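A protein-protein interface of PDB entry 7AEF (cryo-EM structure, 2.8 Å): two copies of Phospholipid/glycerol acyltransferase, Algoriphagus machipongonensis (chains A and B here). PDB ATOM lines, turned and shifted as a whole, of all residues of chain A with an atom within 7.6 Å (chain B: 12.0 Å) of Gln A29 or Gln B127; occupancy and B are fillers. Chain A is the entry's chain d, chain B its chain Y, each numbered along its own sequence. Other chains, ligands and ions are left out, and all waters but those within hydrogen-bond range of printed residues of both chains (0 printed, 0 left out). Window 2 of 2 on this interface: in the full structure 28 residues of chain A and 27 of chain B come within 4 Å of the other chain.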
ATOM      1  N   SER A   9      -4.814  11.449  14.976  1.00  0.00           N
ATOM      2  CA  SER A   9      -3.824  10.404  14.739  1.00  0.00           C
ATOM      3  C   SER A   9      -3.821   9.800  13.332  1.00  0.00           C
ATOM      4  O   SER A   9      -3.159   8.780  13.121  1.00  0.00           O
ATOM      5  CB  SER A   9      -4.039   9.294  15.752  1.00  0.00           C
ATOM      6  OG  SER A   9      -5.339   8.768  15.615  1.00  0.00           O
ATOM      7  N   PHE A  10      -4.511  10.385  12.357  1.00  0.00           N
ATOM      8  CA  PHE A  10      -4.602   9.745  11.047  1.00  0.00           C
ATOM      9  C   PHE A  10      -3.640  10.269   9.974  1.00  0.00           C
ATOM     10  O   PHE A  10      -3.796   9.907   8.806  1.00  0.00           O
ATOM     11  CB  PHE A  10      -6.033   9.796  10.506  1.00  0.00           C
ATOM     12  CG  PHE A  10      -6.654  11.154  10.461  1.00  0.00           C
ATOM     13  CD1 PHE A  10      -6.405  12.023   9.421  1.00  0.00           C
ATOM     14  CD2 PHE A  10      -7.555  11.530  11.427  1.00  0.00           C
ATOM     15  CE1 PHE A  10      -7.006  13.242   9.371  1.00  0.00           C
ATOM     16  CE2 PHE A  10      -8.166  12.750  11.370  1.00  0.00           C
ATOM     17  CZ  PHE A  10      -7.887  13.608  10.340  1.00  0.00           C
ATOM     18  N   PHE A  12       0.448  10.514   9.153  1.00  0.00           N
ATOM     19  CA  PHE A  12       1.784  10.094   9.576  1.00  0.00           C
ATOM     20  C   PHE A  12       2.605   9.473   8.436  1.00  0.00           C
ATOM     21  O   PHE A  12       2.057   9.018   7.434  1.00  0.00           O
ATOM     22  CB  PHE A  12       1.668   9.089  10.730  1.00  0.00           C
ATOM     23  CG  PHE A  12       0.836   7.867  10.393  1.00  0.00           C
ATOM     24  CD1 PHE A  12       1.406   6.732   9.841  1.00  0.00           C
ATOM     25  CD2 PHE A  12      -0.522   7.855  10.633  1.00  0.00           C
ATOM     26  CE1 PHE A  12       0.625   5.642   9.510  1.00  0.00           C
ATOM     27  CE2 PHE A  12      -1.288   6.758  10.318  1.00  0.00           C
ATOM     28  CZ  PHE A  12      -0.706   5.648   9.763  1.00  0.00           C
ATOM     29  N   HIS A  26       6.824   3.941   1.886  1.00  0.00           N
ATOM     30  CA  HIS A  26       6.670   4.858   2.997  1.00  0.00           C
ATOM     31  C   HIS A  26       5.235   5.014   3.411  1.00  0.00           C
ATOM     32  O   HIS A  26       4.960   5.778   4.325  1.00  0.00           O
ATOM     33  CB  HIS A  26       7.215   6.234   2.660  1.00  0.00           C
ATOM     34  CG  HIS A  26       8.678   6.251   2.389  1.00  0.00           C
ATOM     35  ND1 HIS A  26       9.533   5.275   2.845  1.00  0.00           N
ATOM     36  CD2 HIS A  26       9.441   7.141   1.718  1.00  0.00           C
ATOM     37  CE1 HIS A  26      10.762   5.557   2.459  1.00  0.00           C
ATOM     38  NE2 HIS A  26      10.733   6.684   1.773  1.00  0.00           N
ATOM     39  N   GLU A  27       4.317   4.317   2.769  1.00  0.00           N
ATOM     40  CA  GLU A  27       2.898   4.487   3.035  1.00  0.00           C
ATOM     41  C   GLU A  27       2.294   3.283   3.743  1.00  0.00           C
ATOM     42  O   GLU A  27       2.313   2.172   3.214  1.00  0.00           O
ATOM     43  CB  GLU A  27       2.178   4.745   1.727  1.00  0.00           C
ATOM     44  CG  GLU A  27       2.942   5.699   0.851  1.00  0.00           C
ATOM     45  CD  GLU A  27       2.469   5.666  -0.570  1.00  0.00           C
ATOM     46  OE1 GLU A  27       1.703   4.741  -0.906  1.00  0.00           O
ATOM     47  OE2 GLU A  27       2.864   6.558  -1.351  1.00  0.00           O
ATOM     48  N   PHE A  28       1.703   3.518   4.910  1.00  0.00           N
ATOM     49  CA  PHE A  28       1.141   2.439   5.700  1.00  0.00           C
ATOM     50  C   PHE A  28      -0.270   2.749   6.165  1.00  0.00           C
ATOM     51  O   PHE A  28      -0.672   3.900   6.295  1.00  0.00           O
ATOM     52  CB  PHE A  28       2.042   2.116   6.885  1.00  0.00           C
ATOM     53  CG  PHE A  28       3.276   1.380   6.495  1.00  0.00           C
ATOM     54  CD1 PHE A  28       4.454   2.058   6.221  1.00  0.00           C
ATOM     55  CD2 PHE A  28       3.250   0.013   6.355  1.00  0.00           C
ATOM     56  CE1 PHE A  28       5.583   1.376   5.839  1.00  0.00           C
ATOM     57  CE2 PHE A  28       4.371  -0.670   5.973  1.00  0.00           C
ATOM     58  CZ  PHE A  28       5.538   0.012   5.715  1.00  0.00           C
ATOM     59  N   GLN A  29      -1.031   1.669   6.325  1.00  0.00           N
ATOM     60  CA  GLN A  29      -2.386   1.715   6.868  1.00  0.00           C
ATOM     61  C   GLN A  29      -2.392   1.935   8.379  1.00  0.00           C
ATOM     62  O   GLN A  29      -3.254   2.661   8.901  1.00  0.00           O
ATOM     63  CB  GLN A  29      -3.117   0.413   6.526  1.00  0.00           C
ATOM     64  CG  GLN A  29      -4.516   0.317   7.099  1.00  0.00           C
ATOM     65  CD  GLN A  29      -5.199  -0.993   6.777  1.00  0.00           C
ATOM     66  OE1 GLN A  29      -4.653  -1.829   6.065  1.00  0.00           O
ATOM     67  NE2 GLN A  29      -6.404  -1.174   7.301  1.00  0.00           N
ATOM     68  N   SER A  30      -1.441   1.310   9.096  1.00  0.00           N
ATOM     69  CA  SER A  30      -1.444   1.405  10.549  1.00  0.00           C
ATOM     70  C   SER A  30      -0.051   1.115  11.130  1.00  0.00           C
ATOM     71  O   SER A  30       0.722   0.323  10.582  1.00  0.00           O
ATOM     72  CB  SER A  30      -2.447   0.425  11.132  1.00  0.00           C
ATOM     73  OG  SER A  30      -2.311   0.377  12.521  1.00  0.00           O
ATOM     74  N   VAL A  31       0.247   1.768  12.260  1.00  0.00           N
ATOM     75  CA  VAL A  31       1.508   1.623  12.997  1.00  0.00           C
ATOM     76  C   VAL A  31       1.192   1.351  14.462  1.00  0.00           C
ATOM     77  O   VAL A  31       0.384   2.067  15.044  1.00  0.00           O
ATOM     78  CB  VAL A  31       2.365   2.901  12.954  1.00  0.00           C
ATOM     79  CG1 VAL A  31       3.790   2.604  13.370  1.00  0.00           C
ATOM     80  CG2 VAL A  31       2.299   3.584  11.651  1.00  0.00           C
ATOM     81  N   LEU A  66       3.709  -2.974  11.546  1.00  0.00           N
ATOM     82  CA  LEU A  66       3.269  -2.192  10.399  1.00  0.00           C
ATOM     83  C   LEU A  66       2.294  -2.963   9.502  1.00  0.00           C
ATOM     84  O   LEU A  66       2.538  -4.124   9.165  1.00  0.00           O
ATOM     85  CB  LEU A  66       4.489  -1.764   9.578  1.00  0.00           C
ATOM     86  CG  LEU A  66       5.592  -0.945  10.274  1.00  0.00           C
ATOM     87  CD1 LEU A  66       6.772  -0.766   9.351  1.00  0.00           C
ATOM     88  CD2 LEU A  66       5.061   0.396  10.667  1.00  0.00           C
ATOM     89  N   LYS A  67       1.216  -2.302   9.052  1.00  0.00           N
ATOM     90  CA  LYS A  67       0.268  -2.915   8.115  1.00  0.00           C
ATOM     91  C   LYS A  67       0.007  -2.051   6.887  1.00  0.00           C
ATOM     92  O   LYS A  67       0.023  -0.821   6.964  1.00  0.00           O
ATOM     93  CB  LYS A  67      -1.074  -3.200   8.769  1.00  0.00           C
ATOM     94  CG  LYS A  67      -1.025  -4.245   9.827  1.00  0.00           C
ATOM     95  CD  LYS A  67      -2.399  -4.515  10.369  1.00  0.00           C
ATOM     96  CE  LYS A  67      -2.367  -5.581  11.439  1.00  0.00           C
ATOM     97  NZ  LYS A  67      -3.715  -5.808  12.040  1.00  0.00           N
ATOM     98  N   ARG A  68      -0.281  -2.719   5.761  1.00  0.00           N
ATOM     99  CA  ARG A  68      -0.607  -2.073   4.486  1.00  0.00           C
ATOM    100  C   ARG A  68      -1.222  -3.071   3.505  1.00  0.00           C
ATOM    101  O   ARG A  68      -1.181  -4.278   3.728  1.00  0.00           O
ATOM    102  CB  ARG A  68       0.633  -1.478   3.855  1.00  0.00           C
ATOM    103  CG  ARG A  68       1.622  -2.529   3.467  1.00  0.00           C
ATOM    104  CD  ARG A  68       2.790  -1.936   2.844  1.00  0.00           C
ATOM    105  NE  ARG A  68       3.663  -2.982   2.367  1.00  0.00           N
ATOM    106  CZ  ARG A  68       4.867  -2.789   1.859  1.00  0.00           C
ATOM    107  NH1 ARG A  68       5.389  -1.575   1.760  1.00  0.00           N
ATOM    108  NH2 ARG A  68       5.535  -3.842   1.446  1.00  0.00           N
ATOM    109  N   GLY A  69      -1.755  -2.561   2.388  1.00  0.00           N
ATOM    110  CA  GLY A  69      -2.186  -3.446   1.311  1.00  0.00           C
ATOM    111  C   GLY A  69      -0.984  -4.088   0.648  1.00  0.00           C
ATOM    112  O   GLY A  69       0.097  -3.518   0.638  1.00  0.00           O
ATOM    113  N   GLU A 122      -2.947 -12.022   5.167  1.00  0.00           N
ATOM    114  CA  GLU A 122      -4.231 -12.525   5.648  1.00  0.00           C
ATOM    115  C   GLU A 122      -4.905 -13.488   4.666  1.00  0.00           C
ATOM    116  O   GLU A 122      -4.694 -13.429   3.455  1.00  0.00           O
ATOM    117  CB  GLU A 122      -5.168 -11.357   5.955  1.00  0.00           C
ATOM    118  CG  GLU A 122      -4.687 -10.515   7.117  1.00  0.00           C
ATOM    119  CD  GLU A 122      -5.665  -9.477   7.557  1.00  0.00           C
ATOM    120  OE1 GLU A 122      -6.685  -9.304   6.893  1.00  0.00           O
ATOM    121  OE2 GLU A 122      -5.368  -8.761   8.519  1.00  0.00           O
ATOM    122  N   MET A 131      -9.698  -6.558   0.443  1.00  0.00           N
ATOM    123  CA  MET A 131      -8.355  -6.280  -0.042  1.00  0.00           C
ATOM    124  C   MET A 131      -7.362  -7.229   0.609  1.00  0.00           C
ATOM    125  O   MET A 131      -7.506  -7.570   1.779  1.00  0.00           O
ATOM    126  CB  MET A 131      -7.992  -4.836   0.284  1.00  0.00           C
ATOM    127  CG  MET A 131      -6.645  -4.388  -0.205  1.00  0.00           C
ATOM    128  SD  MET A 131      -6.324  -2.677   0.161  1.00  0.00           S
ATOM    129  CE  MET A 131      -7.332  -1.843  -1.053  1.00  0.00           C
ATOM    130  N   ALA A 132      -6.344  -7.647  -0.136  1.00  0.00           N
ATOM    131  CA  ALA A 132      -5.292  -8.454   0.466  1.00  0.00           C
ATOM    132  C   ALA A 132      -4.386  -7.573   1.315  1.00  0.00           C
ATOM    133  O   ALA A 132      -3.831  -6.588   0.822  1.00  0.00           O
ATOM    134  CB  ALA A 132      -4.481  -9.174  -0.602  1.00  0.00           C
ATOM    135  N   ILE A 133      -4.225  -7.944   2.588  1.00  0.00           N
ATOM    136  CA  ILE A 133      -3.471  -7.158   3.562  1.00  0.00           C
ATOM    137  C   ILE A 133      -2.208  -7.881   4.019  1.00  0.00           C
ATOM    138  O   ILE A 133      -2.237  -9.065   4.393  1.00  0.00           O
ATOM    139  CB  ILE A 133      -4.340  -6.770   4.771  1.00  0.00           C
ATOM    140  CG1 ILE A 133      -5.583  -5.977   4.312  1.00  0.00           C
ATOM    141  CG2 ILE A 133      -3.534  -5.985   5.827  1.00  0.00           C
ATOM    142  CD1 ILE A 133      -5.324  -4.669   3.561  1.00  0.00           C
ATOM    143  N   GLU A 134      -1.108  -7.122   4.035  1.00  0.00           N
ATOM    144  CA  GLU A 134       0.202  -7.596   4.431  1.00  0.00           C
ATOM    145  C   GLU A 134       0.598  -7.005   5.793  1.00  0.00           C
ATOM    146  O   GLU A 134       0.270  -5.858   6.120  1.00  0.00           O
ATOM    147  CB  GLU A 134       1.201  -7.242   3.340  1.00  0.00           C
ATOM    148  CG  GLU A 134       2.618  -7.443   3.670  1.00  0.00           C
ATOM    149  CD  GLU A 134       3.425  -7.273   2.465  1.00  0.00           C
ATOM    150  OE1 GLU A 134       3.598  -6.124   2.056  1.00  0.00           O
ATOM    151  OE2 GLU A 134       4.046  -8.237   2.027  1.00  0.00           O
ATOM    152  N   GLU B 122      -1.477   5.467  22.111  1.00  0.00           N
ATOM    153  CA  GLU B 122      -2.314   4.530  21.366  1.00  0.00           C
ATOM    154  C   GLU B 122      -2.030   4.536  19.860  1.00  0.00           C
ATOM    155  O   GLU B 122      -1.582   5.533  19.292  1.00  0.00           O
ATOM    156  CB  GLU B 122      -3.791   4.834  21.616  1.00  0.00           C
ATOM    157  CG  GLU B 122      -4.202   4.576  23.050  1.00  0.00           C
ATOM    158  CD  GLU B 122      -5.673   4.690  23.285  1.00  0.00           C
ATOM    159  OE1 GLU B 122      -6.390   5.094  22.372  1.00  0.00           O
ATOM    160  OE2 GLU B 122      -6.103   4.468  24.421  1.00  0.00           O
ATOM    161  N   ASP B 123      -2.340   3.400  19.223  1.00  0.00           N
ATOM    162  CA  ASP B 123      -2.085   3.122  17.807  1.00  0.00           C
ATOM    163  C   ASP B 123      -2.686   4.144  16.846  1.00  0.00           C
ATOM    164  O   ASP B 123      -3.793   4.650  17.038  1.00  0.00           O
ATOM    165  CB  ASP B 123      -2.693   1.784  17.397  1.00  0.00           C
ATOM    166  CG  ASP B 123      -2.005   0.587  17.981  1.00  0.00           C
ATOM    167  OD1 ASP B 123      -0.952   0.699  18.595  1.00  0.00           O
ATOM    168  OD2 ASP B 123      -2.547  -0.505  17.810  1.00  0.00           O
ATOM    169  N   PHE B 124      -1.972   4.365  15.757  1.00  0.00           N
ATOM    170  CA  PHE B 124      -2.397   5.253  14.693  1.00  0.00           C
ATOM    171  C   PHE B 124      -3.194   4.453  13.675  1.00  0.00           C
ATOM    172  O   PHE B 124      -2.886   3.290  13.424  1.00  0.00           O
ATOM    173  CB  PHE B 124      -1.181   5.879  14.018  1.00  0.00           C
ATOM    174  CG  PHE B 124      -0.320   6.729  14.929  1.00  0.00           C
ATOM    175  CD1 PHE B 124       0.974   6.999  14.561  1.00  0.00           C
ATOM    176  CD2 PHE B 124      -0.782   7.251  16.136  1.00  0.00           C
ATOM    177  CE1 PHE B 124       1.795   7.764  15.358  1.00  0.00           C
ATOM    178  CE2 PHE B 124       0.042   8.006  16.936  1.00  0.00           C
ATOM    179  CZ  PHE B 124       1.329   8.264  16.542  1.00  0.00           C
ATOM    180  N   ASN B 125      -4.214   5.072  13.084  1.00  0.00           N
ATOM    181  CA  ASN B 125      -5.028   4.384  12.082  1.00  0.00           C
ATOM    182  C   ASN B 125      -5.475   5.382  11.023  1.00  0.00           C
ATOM    183  O   ASN B 125      -6.283   6.269  11.289  1.00  0.00           O
ATOM    184  CB  ASN B 125      -6.212   3.686  12.733  1.00  0.00           C
ATOM    185  CG  ASN B 125      -6.997   2.803  11.771  1.00  0.00           C
ATOM    186  OD1 ASN B 125      -7.104   3.034  10.562  1.00  0.00           O
ATOM    187  ND2 ASN B 125      -7.573   1.770  12.327  1.00  0.00           N
ATOM    188  N   ALA B 126      -4.980   5.175   9.806  1.00  0.00           N
ATOM    189  CA  ALA B 126      -5.237   6.054   8.673  1.00  0.00           C
ATOM    190  C   ALA B 126      -6.698   6.117   8.264  1.00  0.00           C
ATOM    191  O   ALA B 126      -7.092   7.044   7.549  1.00  0.00           O
ATOM    192  CB  ALA B 126      -4.431   5.582   7.480  1.00  0.00           C
ATOM    193  N   GLN B 127      -7.494   5.125   8.640  1.00  0.00           N
ATOM    194  CA  GLN B 127      -8.884   5.058   8.231  1.00  0.00           C
ATOM    195  C   GLN B 127      -9.872   5.427   9.335  1.00  0.00           C
ATOM    196  O   GLN B 127     -11.075   5.228   9.153  1.00  0.00           O
ATOM    197  CB  GLN B 127      -9.189   3.663   7.697  1.00  0.00           C
ATOM    198  CG  GLN B 127      -8.418   3.343   6.434  1.00  0.00           C
ATOM    199  CD  GLN B 127      -8.717   1.977   5.888  1.00  0.00           C
ATOM    200  OE1 GLN B 127      -9.855   1.521   5.911  1.00  0.00           O
ATOM    201  NE2 GLN B 127      -7.691   1.310   5.386  1.00  0.00           N
ATOM    202  N   GLU B 128      -9.416   5.975  10.462  1.00  0.00           N
ATOM    203  CA  GLU B 128     -10.341   6.311  11.530  1.00  0.00           C
ATOM    204  C   GLU B 128     -10.141   7.763  11.965  1.00  0.00           C
ATOM    205  O   GLU B 128      -9.027   8.281  11.958  1.00  0.00           O
ATOM    206  CB  GLU B 128     -10.106   5.411  12.730  1.00  0.00           C
ATOM    207  CG  GLU B 128     -10.539   3.977  12.540  1.00  0.00           C
ATOM    208  CD  GLU B 128     -10.326   3.166  13.789  1.00  0.00           C
ATOM    209  OE1 GLU B 128      -9.484   3.548  14.604  1.00  0.00           O
ATOM    210  OE2 GLU B 128     -11.041   2.180  13.993  1.00  0.00           O
ATOM    211  N   SER B 129     -11.214   8.416  12.356  1.00  0.00           N
ATOM    212  CA  SER B 129     -11.152   9.761  12.921  1.00  0.00           C
ATOM    213  C   SER B 129     -11.092   9.741  14.430  1.00  0.00           C
ATOM    214  O   SER B 129     -12.113   9.556  15.090  1.00  0.00           O
ATOM    215  CB  SER B 129     -12.346  10.571  12.460  1.00  0.00           C
ATOM    216  OG  SER B 129     -12.218  11.899  12.887  1.00  0.00           O
ATOM    217  N   LYS B 130      -9.891   9.930  14.984  1.00  0.00           N
ATOM    218  CA  LYS B 130      -9.659   9.808  16.416  1.00  0.00           C
ATOM    219  C   LYS B 130      -8.572  10.763  16.891  1.00  0.00           C
ATOM    220  O   LYS B 130      -7.705  11.181  16.126  1.00  0.00           O
ATOM    221  CB  LYS B 130      -9.251   8.382  16.768  1.00  0.00           C
ATOM    222  CG  LYS B 130     -10.360   7.371  16.698  1.00  0.00           C
ATOM    223  CD  LYS B 130      -9.906   6.011  17.115  1.00  0.00           C
ATOM    224  CE  LYS B 130     -11.011   4.990  16.916  1.00  0.00           C
ATOM    225  NZ  LYS B 130     -10.537   3.600  17.170  1.00  0.00           N
ATOM    226  N   MET B 131      -8.613  11.069  18.181  1.00  0.00           N
ATOM    227  CA  MET B 131      -7.601  11.882  18.839  1.00  0.00           C
ATOM    228  C   MET B 131      -6.456  11.002  19.313  1.00  0.00           C
ATOM    229  O   MET B 131      -6.681   9.874  19.747  1.00  0.00           O
ATOM    230  CB  MET B 131      -8.230  12.606  20.023  1.00  0.00           C
ATOM    231  CG  MET B 131      -7.311  13.527  20.772  1.00  0.00           C
ATOM    232  SD  MET B 131      -8.136  14.380  22.098  1.00  0.00           S
ATOM    233  CE  MET B 131      -9.079  15.613  21.215  1.00  0.00           C
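The backbone carbonyl oxygen (O) of Phe B124 sits at hydrogen-bond distance from the side-chain hydroxyl (OG) of Ser A30 (3.1 Å). The backbone NH (N) of Phe B124 lies within hydrogen-bond range of the backbone carbonyl oxygen (O) of Val A31 (3.4 Å). N of Ala B126 lies within hydrogen-bond range of O of Gln A29 (3.2 Å). The side-chain amide nitrogen (NE2) of Gln A29 lies close to the side-chain amide nitrogen (NE2) of Gln B127 (3.4 Å). The backbone carbonyl oxygen of Lys B130 sits at hydrogen-bond distance from the backbone NH of Ser A9.
The side-chain amide oxygen (OD1) of Asn B125 lies within hydrogen-bond range of the backbone NH (N) of Gln B127. The side-chain amide nitrogen (ND2) of Asn B125 lies close to the side-chain carboxylate (OE1) of Glu B128 (3.5 Å). OE1 of Glu B128 lies within salt-bridge range of NZ of Lys B130. O of Lys A67 is in hydrogen-bond range of N of Gln A29, 2.8 Å away. The backbone carbonyl oxygen of Ser A30 is in hydrogen-bond range of the backbone NH of Lys A67 (3.1 Å).
Among the printed residues, merely in contact across the chains: Phe A10 with Glu B128 (3.6 Å), Phe A10 with Asn B125 (3.6 Å), Ser A9 with Phe B124 (3.6 Å), Phe A12 with Phe B124 (3.8 Å), Val A31 with Asp B123 (3.9 Å) and Ser A9 with Asn B125 (3.9 Å).
Of the printed residues of chain B, Phe A10 touches Asn B125 (3.6 Å) and Glu B128 (3.6 Å). Glu A27 touches none of the printed residues of chain B. Gln A29 touches just these residues of chain B: Ala B126 (3.2 Å) and Gln B127 (3.4 Å). Of chain B, only Phe B124 comes within 4 Å of Ser A30. No residue of chain B comes within 4 Å of Lys A67. No residue of chain B comes within 4 Å of Gly A69. Glu A122 touches none of the printed residues of chain B. No residue of chain B comes within 4 Å of Ile A133. Of the printed residues of chain A, Phe B124 touches Ser A9 (3.6 Å), Phe A12 (3.8 Å), Ser A30 (3.1 Å) and Val A31 (3.4 Å). Of chain A, only Gln A29 (3.2 Å) comes within 4 Å of Ala B126. Gln B127 touches just one residue of chain A: Gln A29 (3.4 Å). The nearest residue of chain A that does not touch Gln B127 is Phe A10 (5.2 Å). The nearest printed residue of chain A that does not touch Asn B125 is Gln A29 (4.03 Å).
Printed residues of chain B that touch a printed residue of chain A: Asp B123, Phe B124, Asn B125, Ala B126, Gln B127, Glu B128 and Lys B130. Hydrophobic or aromatic side chains of chain B within 4 Å of the printed part of chain A: Phe B124 and Ala B126. Of the 18 printed residues of chain A, 6 touch a printed residue of chain B. Hydrophobic or aromatic side chains of chain A within 4 Å of the printed part of chain B: Phe A10 and Phe A12. Among the printed residues, 11 pairs touch across the chains. Among the printed residues, no Asp or Glu carboxylate lies within 4 Å of a Lys or Arg side-chain nitrogen of the other chain.
2 positions are printed for both chains. Of the 11 pairs that touch across the chains among the printed residues, none has its exchanged pair printed and touching as well.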
